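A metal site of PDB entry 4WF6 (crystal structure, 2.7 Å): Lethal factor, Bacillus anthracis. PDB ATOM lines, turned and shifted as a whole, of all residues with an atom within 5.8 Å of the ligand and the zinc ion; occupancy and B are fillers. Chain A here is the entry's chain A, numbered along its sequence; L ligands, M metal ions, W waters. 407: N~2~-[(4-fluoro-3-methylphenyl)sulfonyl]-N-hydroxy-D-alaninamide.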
ATOM      1  N   ASP A  67      12.049  18.340  10.271  1.00  0.00           N
ATOM      2  CA  ASP A  67      12.171  19.681  10.844  1.00  0.00           C
ATOM      3  C   ASP A  67      13.090  19.698  12.062  1.00  0.00           C
ATOM      4  O   ASP A  67      12.982  20.587  12.912  1.00  0.00           O
ATOM      5  CB  ASP A  67      10.786  20.211  11.220  1.00  0.00           C
ATOM      6  CG  ASP A  67      10.067  19.317  12.222  1.00  0.00           C
ATOM      7  OD1 ASP A  67      10.401  18.107  12.280  1.00  0.00           O
ATOM      8  OD2 ASP A  67       9.179  19.808  12.935  1.00  0.00           O
ATOM      9  N   PHE A  68      13.994  18.736  12.138  1.00  0.00           N
ATOM     10  CA  PHE A  68      14.863  18.589  13.301  1.00  0.00           C
ATOM     11  C   PHE A  68      16.303  18.290  12.913  1.00  0.00           C
ATOM     12  O   PHE A  68      17.212  18.359  13.743  1.00  0.00           O
ATOM     13  CB  PHE A  68      14.341  17.480  14.222  1.00  0.00           C
ATOM     14  CG  PHE A  68      14.153  16.166  13.533  1.00  0.00           C
ATOM     15  CD1 PHE A  68      15.137  15.188  13.603  1.00  0.00           C
ATOM     16  CD2 PHE A  68      12.987  15.891  12.829  1.00  0.00           C
ATOM     17  CE1 PHE A  68      14.964  13.963  12.975  1.00  0.00           C
ATOM     18  CE2 PHE A  68      12.814  14.667  12.200  1.00  0.00           C
ATOM     19  CZ  PHE A  68      13.795  13.711  12.275  1.00  0.00           C
ATOM     20  N   VAL A 392      16.823  18.688  19.034  1.00  0.00           N
ATOM     21  CA  VAL A 392      16.328  19.310  17.810  1.00  0.00           C
ATOM     22  C   VAL A 392      17.168  20.494  17.389  1.00  0.00           C
ATOM     23  O   VAL A 392      17.468  21.376  18.206  1.00  0.00           O
ATOM     24  CB  VAL A 392      14.871  19.779  17.980  1.00  0.00           C
ATOM     25  CG1 VAL A 392      14.405  20.524  16.740  1.00  0.00           C
ATOM     26  CG2 VAL A 392      13.959  18.600  18.291  1.00  0.00           C
ATOM     27  N   SER A 394      16.814  23.608  14.642  1.00  0.00           N
ATOM     28  CA  SER A 394      15.793  24.244  13.834  1.00  0.00           C
ATOM     29  C   SER A 394      15.952  25.752  13.900  1.00  0.00           C
ATOM     30  O   SER A 394      16.835  26.257  14.600  1.00  0.00           O
ATOM     31  CB  SER A 394      14.399  23.827  14.312  1.00  0.00           C
ATOM     32  OG  SER A 394      14.252  24.055  15.706  1.00  0.00           O
ATOM     33  N   LYS A 395      15.114  26.470  13.166  1.00  0.00           N
ATOM     34  CA  LYS A 395      15.117  27.930  13.205  1.00  0.00           C
ATOM     35  C   LYS A 395      14.880  28.424  14.618  1.00  0.00           C
ATOM     36  O   LYS A 395      15.623  29.264  15.138  1.00  0.00           O
ATOM     37  CB  LYS A 395      14.060  28.499  12.261  1.00  0.00           C
ATOM     38  CG  LYS A 395      13.943  30.012  12.304  1.00  0.00           C
ATOM     39  CD  LYS A 395      15.256  30.665  11.920  1.00  0.00           C
ATOM     40  CE  LYS A 395      15.175  32.176  12.013  1.00  0.00           C
ATOM     41  NZ  LYS A 395      16.435  32.820  11.557  1.00  0.00           N
ATOM     42  N   GLY A 396      13.840  27.884  15.245  1.00  0.00           N
ATOM     43  CA  GLY A 396      13.462  28.290  16.591  1.00  0.00           C
ATOM     44  C   GLY A 396      12.920  27.128  17.387  1.00  0.00           C
ATOM     45  O   GLY A 396      12.636  26.059  16.826  1.00  0.00           O
ATOM     46  N   LEU A 397      12.777  27.330  18.694  1.00  0.00           N
ATOM     47  CA  LEU A 397      12.348  26.260  19.579  1.00  0.00           C
ATOM     48  C   LEU A 397      11.828  26.819  20.900  1.00  0.00           C
ATOM     49  O   LEU A 397      12.328  27.825  21.401  1.00  0.00           O
ATOM     50  CB  LEU A 397      13.501  25.291  19.841  1.00  0.00           C
ATOM     51  CG  LEU A 397      13.161  23.879  20.302  1.00  0.00           C
ATOM     52  CD1 LEU A 397      12.334  23.170  19.239  1.00  0.00           C
ATOM     53  CD2 LEU A 397      14.433  23.099  20.592  1.00  0.00           C
ATOM     54  N   TYR A 398      10.792  26.186  21.445  1.00  0.00           N
ATOM     55  CA  TYR A 398      10.378  26.482  22.810  1.00  0.00           C
ATOM     56  C   TYR A 398      10.582  25.246  23.684  1.00  0.00           C
ATOM     57  O   TYR A 398      10.130  24.147  23.345  1.00  0.00           O
ATOM     58  CB  TYR A 398       8.924  26.927  22.882  1.00  0.00           C
ATOM     59  CG  TYR A 398       8.439  27.117  24.307  1.00  0.00           C
ATOM     60  CD1 TYR A 398       8.909  28.175  25.076  1.00  0.00           C
ATOM     61  CD2 TYR A 398       7.545  26.232  24.886  1.00  0.00           C
ATOM     62  CE1 TYR A 398       8.484  28.357  26.385  1.00  0.00           C
ATOM     63  CE2 TYR A 398       7.117  26.405  26.194  1.00  0.00           C
ATOM     64  CZ  TYR A 398       7.595  27.466  26.932  1.00  0.00           C
ATOM     65  OH  TYR A 398       7.170  27.648  28.242  1.00  0.00           O
ATOM     66  N   LYS A 412      16.827  29.551   8.302  1.00  0.00           N
ATOM     67  CA  LYS A 412      15.530  30.049   7.850  1.00  0.00           C
ATOM     68  C   LYS A 412      14.436  29.014   8.084  1.00  0.00           C
ATOM     69  O   LYS A 412      14.574  27.859   7.688  1.00  0.00           O
ATOM     70  CB  LYS A 412      15.584  30.424   6.363  1.00  0.00           C
ATOM     71  CG  LYS A 412      14.330  31.105   5.837  1.00  0.00           C
ATOM     72  N   GLY A 413      13.369  29.426   8.754  1.00  0.00           N
ATOM     73  CA  GLY A 413      12.251  28.534   9.020  1.00  0.00           C
ATOM     74  C   GLY A 413      11.400  28.345   7.783  1.00  0.00           C
ATOM     75  O   GLY A 413      11.539  29.082   6.803  1.00  0.00           O
ATOM     76  N   VAL A 414      10.528  27.341   7.804  1.00  0.00           N
ATOM     77  CA  VAL A 414       9.670  27.070   6.662  1.00  0.00           C
ATOM     78  C   VAL A 414       8.637  28.186   6.480  1.00  0.00           C
ATOM     79  O   VAL A 414       7.982  28.610   7.428  1.00  0.00           O
ATOM     80  CB  VAL A 414       8.950  25.700   6.784  1.00  0.00           C
ATOM     81  CG1 VAL A 414       9.969  24.559   6.798  1.00  0.00           C
ATOM     82  CG2 VAL A 414       8.079  25.641   8.032  1.00  0.00           C
ATOM     83  N   LEU A 416       8.621  31.346   6.273  1.00  0.00           N
ATOM     84  CA  LEU A 416       8.669  32.555   7.086  1.00  0.00           C
ATOM     85  C   LEU A 416       9.299  33.698   6.283  1.00  0.00           C
ATOM     86  O   LEU A 416      10.135  33.472   5.424  1.00  0.00           O
ATOM     87  CB  LEU A 416       9.465  32.310   8.373  1.00  0.00           C
ATOM     88  CG  LEU A 416       8.915  31.238   9.322  1.00  0.00           C
ATOM     89  CD1 LEU A 416       9.740  31.179  10.598  1.00  0.00           C
ATOM     90  CD2 LEU A 416       7.451  31.484   9.639  1.00  0.00           C
ATOM     91  N   GLU A 421       8.775  36.568  12.678  1.00  0.00           N
ATOM     92  CA  GLU A 421       7.663  35.637  12.496  1.00  0.00           C
ATOM     93  C   GLU A 421       7.960  34.318  13.196  1.00  0.00           C
ATOM     94  O   GLU A 421       7.055  33.650  13.689  1.00  0.00           O
ATOM     95  CB  GLU A 421       7.385  35.393  11.018  1.00  0.00           C
ATOM     96  CG  GLU A 421       6.683  36.542  10.322  1.00  0.00           C
ATOM     97  CD  GLU A 421       6.121  36.144   8.971  1.00  0.00           C
ATOM     98  OE1 GLU A 421       6.547  35.101   8.428  1.00  0.00           O
ATOM     99  OE2 GLU A 421       5.248  36.883   8.458  1.00  0.00           O
ATOM    100  N   GLY A 422       9.240  33.952  13.247  1.00  0.00           N
ATOM    101  CA  GLY A 422       9.644  32.740  13.926  1.00  0.00           C
ATOM    102  C   GLY A 422       9.509  32.843  15.436  1.00  0.00           C
ATOM    103  O   GLY A 422       9.040  31.912  16.086  1.00  0.00           O
ATOM    104  N   HIS A 425       5.930  32.585  16.630  1.00  0.00           N
ATOM    105  CA  HIS A 425       5.568  31.176  16.642  1.00  0.00           C
ATOM    106  C   HIS A 425       5.967  30.523  17.964  1.00  0.00           C
ATOM    107  O   HIS A 425       5.185  29.779  18.561  1.00  0.00           O
ATOM    108  CB  HIS A 425       6.237  30.448  15.464  1.00  0.00           C
ATOM    109  CG  HIS A 425       6.106  28.963  15.505  1.00  0.00           C
ATOM    110  ND1 HIS A 425       5.282  28.262  14.658  1.00  0.00           N
ATOM    111  CD2 HIS A 425       6.729  28.033  16.270  1.00  0.00           C
ATOM    112  CE1 HIS A 425       5.383  26.965  14.908  1.00  0.00           C
ATOM    113  NE2 HIS A 425       6.250  26.802  15.884  1.00  0.00           N
ATOM    114  N   GLU A 426       7.192  30.800  18.401  1.00  0.00           N
ATOM    115  CA  GLU A 426       7.703  30.193  19.628  1.00  0.00           C
ATOM    116  C   GLU A 426       6.980  30.746  20.852  1.00  0.00           C
ATOM    117  O   GLU A 426       6.733  30.007  21.814  1.00  0.00           O
ATOM    118  CB  GLU A 426       9.210  30.423  19.752  1.00  0.00           C
ATOM    119  CG  GLU A 426      10.009  30.076  18.499  1.00  0.00           C
ATOM    120  CD  GLU A 426       9.844  28.627  18.057  1.00  0.00           C
ATOM    121  OE1 GLU A 426      10.161  28.335  16.891  1.00  0.00           O
ATOM    122  OE2 GLU A 426       9.402  27.793  18.871  1.00  0.00           O
ATOM    123  N   HIS A 429       3.957  28.846  21.512  1.00  0.00           N
ATOM    124  CA  HIS A 429       4.174  27.642  22.311  1.00  0.00           C
ATOM    125  C   HIS A 429       4.141  27.961  23.803  1.00  0.00           C
ATOM    126  O   HIS A 429       3.636  27.163  24.606  1.00  0.00           O
ATOM    127  CB  HIS A 429       5.511  26.996  21.952  1.00  0.00           C
ATOM    128  CG  HIS A 429       5.519  26.296  20.624  1.00  0.00           C
ATOM    129  ND1 HIS A 429       4.570  25.363  20.273  1.00  0.00           N
ATOM    130  CD2 HIS A 429       6.370  26.395  19.579  1.00  0.00           C
ATOM    131  CE1 HIS A 429       4.832  24.918  19.054  1.00  0.00           C
ATOM    132  NE2 HIS A 429       5.921  25.521  18.614  1.00  0.00           N
ATOM    133  N   TYR A 467       2.963  23.318   7.469  1.00  0.00           N
ATOM    134  CA  TYR A 467       3.696  22.972   8.675  1.00  0.00           C
ATOM    135  C   TYR A 467       2.754  22.839   9.878  1.00  0.00           C
ATOM    136  O   TYR A 467       3.038  22.112  10.819  1.00  0.00           O
ATOM    137  CB  TYR A 467       4.790  24.002   8.982  1.00  0.00           C
ATOM    138  CG  TYR A 467       5.602  23.638  10.192  1.00  0.00           C
ATOM    139  CD1 TYR A 467       6.518  22.589  10.146  1.00  0.00           C
ATOM    140  CD2 TYR A 467       5.445  24.309  11.395  1.00  0.00           C
ATOM    141  CE1 TYR A 467       7.261  22.237  11.258  1.00  0.00           C
ATOM    142  CE2 TYR A 467       6.183  23.967  12.520  1.00  0.00           C
ATOM    143  CZ  TYR A 467       7.089  22.927  12.445  1.00  0.00           C
ATOM    144  OH  TYR A 467       7.829  22.568  13.546  1.00  0.00           O
ATOM    145  N   GLU A 474       2.037  22.445  16.976  1.00  0.00           N
ATOM    146  CA  GLU A 474       2.539  23.308  15.921  1.00  0.00           C
ATOM    147  C   GLU A 474       1.408  24.055  15.232  1.00  0.00           C
ATOM    148  O   GLU A 474       1.582  25.188  14.786  1.00  0.00           O
ATOM    149  CB  GLU A 474       3.354  22.497  14.896  1.00  0.00           C
ATOM    150  CG  GLU A 474       4.495  21.678  15.497  1.00  0.00           C
ATOM    151  CD  GLU A 474       5.611  22.530  16.103  1.00  0.00           C
ATOM    152  OE1 GLU A 474       6.517  21.951  16.732  1.00  0.00           O
ATOM    153  OE2 GLU A 474       5.585  23.772  15.942  1.00  0.00           O
ATOM    154  N   ALA A 477       0.523  26.947  17.231  1.00  0.00           N
ATOM    155  CA  ALA A 477       1.608  27.915  17.125  1.00  0.00           C
ATOM    156  C   ALA A 477       1.563  28.650  15.791  1.00  0.00           C
ATOM    157  O   ALA A 477       1.803  29.861  15.739  1.00  0.00           O
ATOM    158  CB  ALA A 477       2.941  27.224  17.299  1.00  0.00           C
ATOM    159  N   GLU A 478       1.252  27.933  14.723  1.00  0.00           N
ATOM    160  CA  GLU A 478       1.140  28.527  13.401  1.00  0.00           C
ATOM    161  C   GLU A 478      -0.075  29.449  13.315  1.00  0.00           C
ATOM    162  O   GLU A 478      -0.004  30.552  12.773  1.00  0.00           O
ATOM    163  CB  GLU A 478       1.053  27.441  12.319  1.00  0.00           C
ATOM    164  CG  GLU A 478       2.403  26.838  11.939  1.00  0.00           C
ATOM    165  CD  GLU A 478       3.323  27.833  11.250  1.00  0.00           C
ATOM    166  OE1 GLU A 478       3.412  27.800  10.002  1.00  0.00           O
ATOM    167  OE2 GLU A 478       3.951  28.654  11.953  1.00  0.00           O
ATOM    168  N   ARG A 481       0.710  32.444  15.149  1.00  0.00           N
ATOM    169  CA  ARG A 481       1.620  33.250  14.348  1.00  0.00           C
ATOM    170  C   ARG A 481       0.839  34.118  13.368  1.00  0.00           C
ATOM    171  O   ARG A 481       0.978  35.336  13.352  1.00  0.00           O
ATOM    172  CB  ARG A 481       2.600  32.345  13.605  1.00  0.00           C
ATOM    173  CG  ARG A 481       3.607  33.106  12.750  1.00  0.00           C
ATOM    174  CD  ARG A 481       4.657  32.178  12.154  1.00  0.00           C
ATOM    175  NE  ARG A 481       4.110  31.234  11.176  1.00  0.00           N
ATOM    176  CZ  ARG A 481       3.906  31.538   9.896  1.00  0.00           C
ATOM    177  NH1 ARG A 481       4.178  32.747   9.434  1.00  0.00           N
ATOM    178  NH2 ARG A 481       3.413  30.620   9.066  1.00  0.00           N
HETATM  179  C1  407 L   1       9.703  24.498  15.746  1.00  0.00           C
HETATM  180  C2  407 L   1      10.699  23.851  14.823  1.00  0.00           C
HETATM  181  N3  407 L   1      10.148  24.991  16.885  1.00  0.00           N
HETATM  182  O4  407 L   1       8.524  24.547  15.429  1.00  0.00           O
HETATM  183  O5  407 L   1       9.255  25.612  17.759  1.00  0.00           O
HETATM  184  C6  407 L   1      10.807  22.363  15.144  1.00  0.00           C
HETATM  185  N7  407 L   1      10.337  24.061  13.435  1.00  0.00           N
HETATM  186  S8  407 L   1      10.955  25.294  12.631  1.00  0.00           S
HETATM  187  O9  407 L   1      11.213  24.912  11.273  1.00  0.00           O
HETATM  188  O10 407 L   1      12.185  25.727  13.245  1.00  0.00           O
HETATM  189  C18 407 L   1       9.908  26.504  12.644  1.00  0.00           C
HETATM  190  C19 407 L   1       8.855  26.537  11.726  1.00  0.00           C
HETATM  191  C20 407 L   1       7.967  27.611  11.756  1.00  0.00           C
HETATM  192  C21 407 L   1       8.121  28.632  12.669  1.00  0.00           C
HETATM  193  C22 407 L   1       9.174  28.602  13.577  1.00  0.00           C
HETATM  194  C23 407 L   1      10.069  27.546  13.550  1.00  0.00           C
HETATM  195  F24 407 L   1       7.258  29.659  12.678  1.00  0.00           F
HETATM  196  C25 407 L   1       6.818  27.659  10.773  1.00  0.00           C
HETATM  197 ZN    ZN M   1       7.069  24.905  16.865  1.00  0.00          ZN
HETATM  198  O   HOH W   1       5.047  27.902   7.975  1.00  0.00           O
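A nitrogen (N3) of the ligand is in hydrogen-bond range of the side-chain carboxylate (OE1) of Glu 426 (3.3 Å).
An oxygen (O10) of the ligand lies within hydrogen-bond range of the backbone NH (N) of Gly 396 (3.4 Å).
O of Gly 396 lies within hydrogen-bond range of N3 of the ligand (2.7 Å).
The side-chain hydroxyl (OH) of Tyr 467 lies within hydrogen-bond range of a nitrogen (N7) of the ligand.
An oxygen (O10) of the ligand lies within hydrogen-bond range of the backbone NH (N) of Lys 395 (3.0 Å).
The side-chain carboxylate of Glu 474 sits close to the side-chain hydroxyl of Tyr 467, at 3.5 Å.
A ring nitrogen (ND1) of His 425 sits at hydrogen-bond distance from the side-chain carboxylate (OE2) of Glu 478, at 3.0 Å.
The backbone NH of Leu 397 lies close to the side-chain carboxylate of Glu 426.
The side-chain carboxylate of Glu 426 lies within hydrogen-bond range of the backbone NH of Tyr 398.
OG of Ser 394 is in hydrogen-bond range of O of Gly 396, 2.8 Å away.
The side-chain carboxylate (OD2) of Asp 67 sits at hydrogen-bond distance from the side-chain hydroxyl (OH) of Tyr 467, at 3.1 Å.
The side-chain carboxylate (OE2) of Glu 478 lies within salt-bridge range of the guanidinium group (NE) of Arg 481 (2.7 Å).
The guanidinium group of Arg 481 lies within salt-bridge range of the side-chain carboxylate of Glu 421, at 3.5 Å.
Asp 67 touches the ligand (O to C6, 3.6 Å).
CB of Ser 394 touches O10 of the ligand (3.1 Å).
CA of Leu 397 touches O5 of the ligand, 3.6 Å away.
Val 414 touches the ligand (CG2 to C25, 3.6 Å).
Leu 416 touches the ligand.
OE2 of Glu 478 touches C25 of the ligand, at 3.3 Å.
Arg 481 touches the ligand.
Hydrophobic or aromatic side chains that line the ligand: Leu 397, Val 414, Leu 416, His 425, His 429 and Tyr 467.
Within 4 Å of the zinc ion: His 425, His 429 and Glu 474.
The zinc ion is bound by O4 of the ligand (2.1 Å), OE2 of Glu 474 (2.1 Å), NE2 of His 429 (2.2 Å), NE2 of His 425 (2.3 Å) and O5 of the ligand (2.5 Å).
The zinc ion has five donor atoms within binding distance.
Water W1 lies within hydrogen-bond range of OE1 of Glu 478 (2.6 Å), O of Val 414 (3.1 Å) and NH2 of Arg 481 (3.4 Å).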
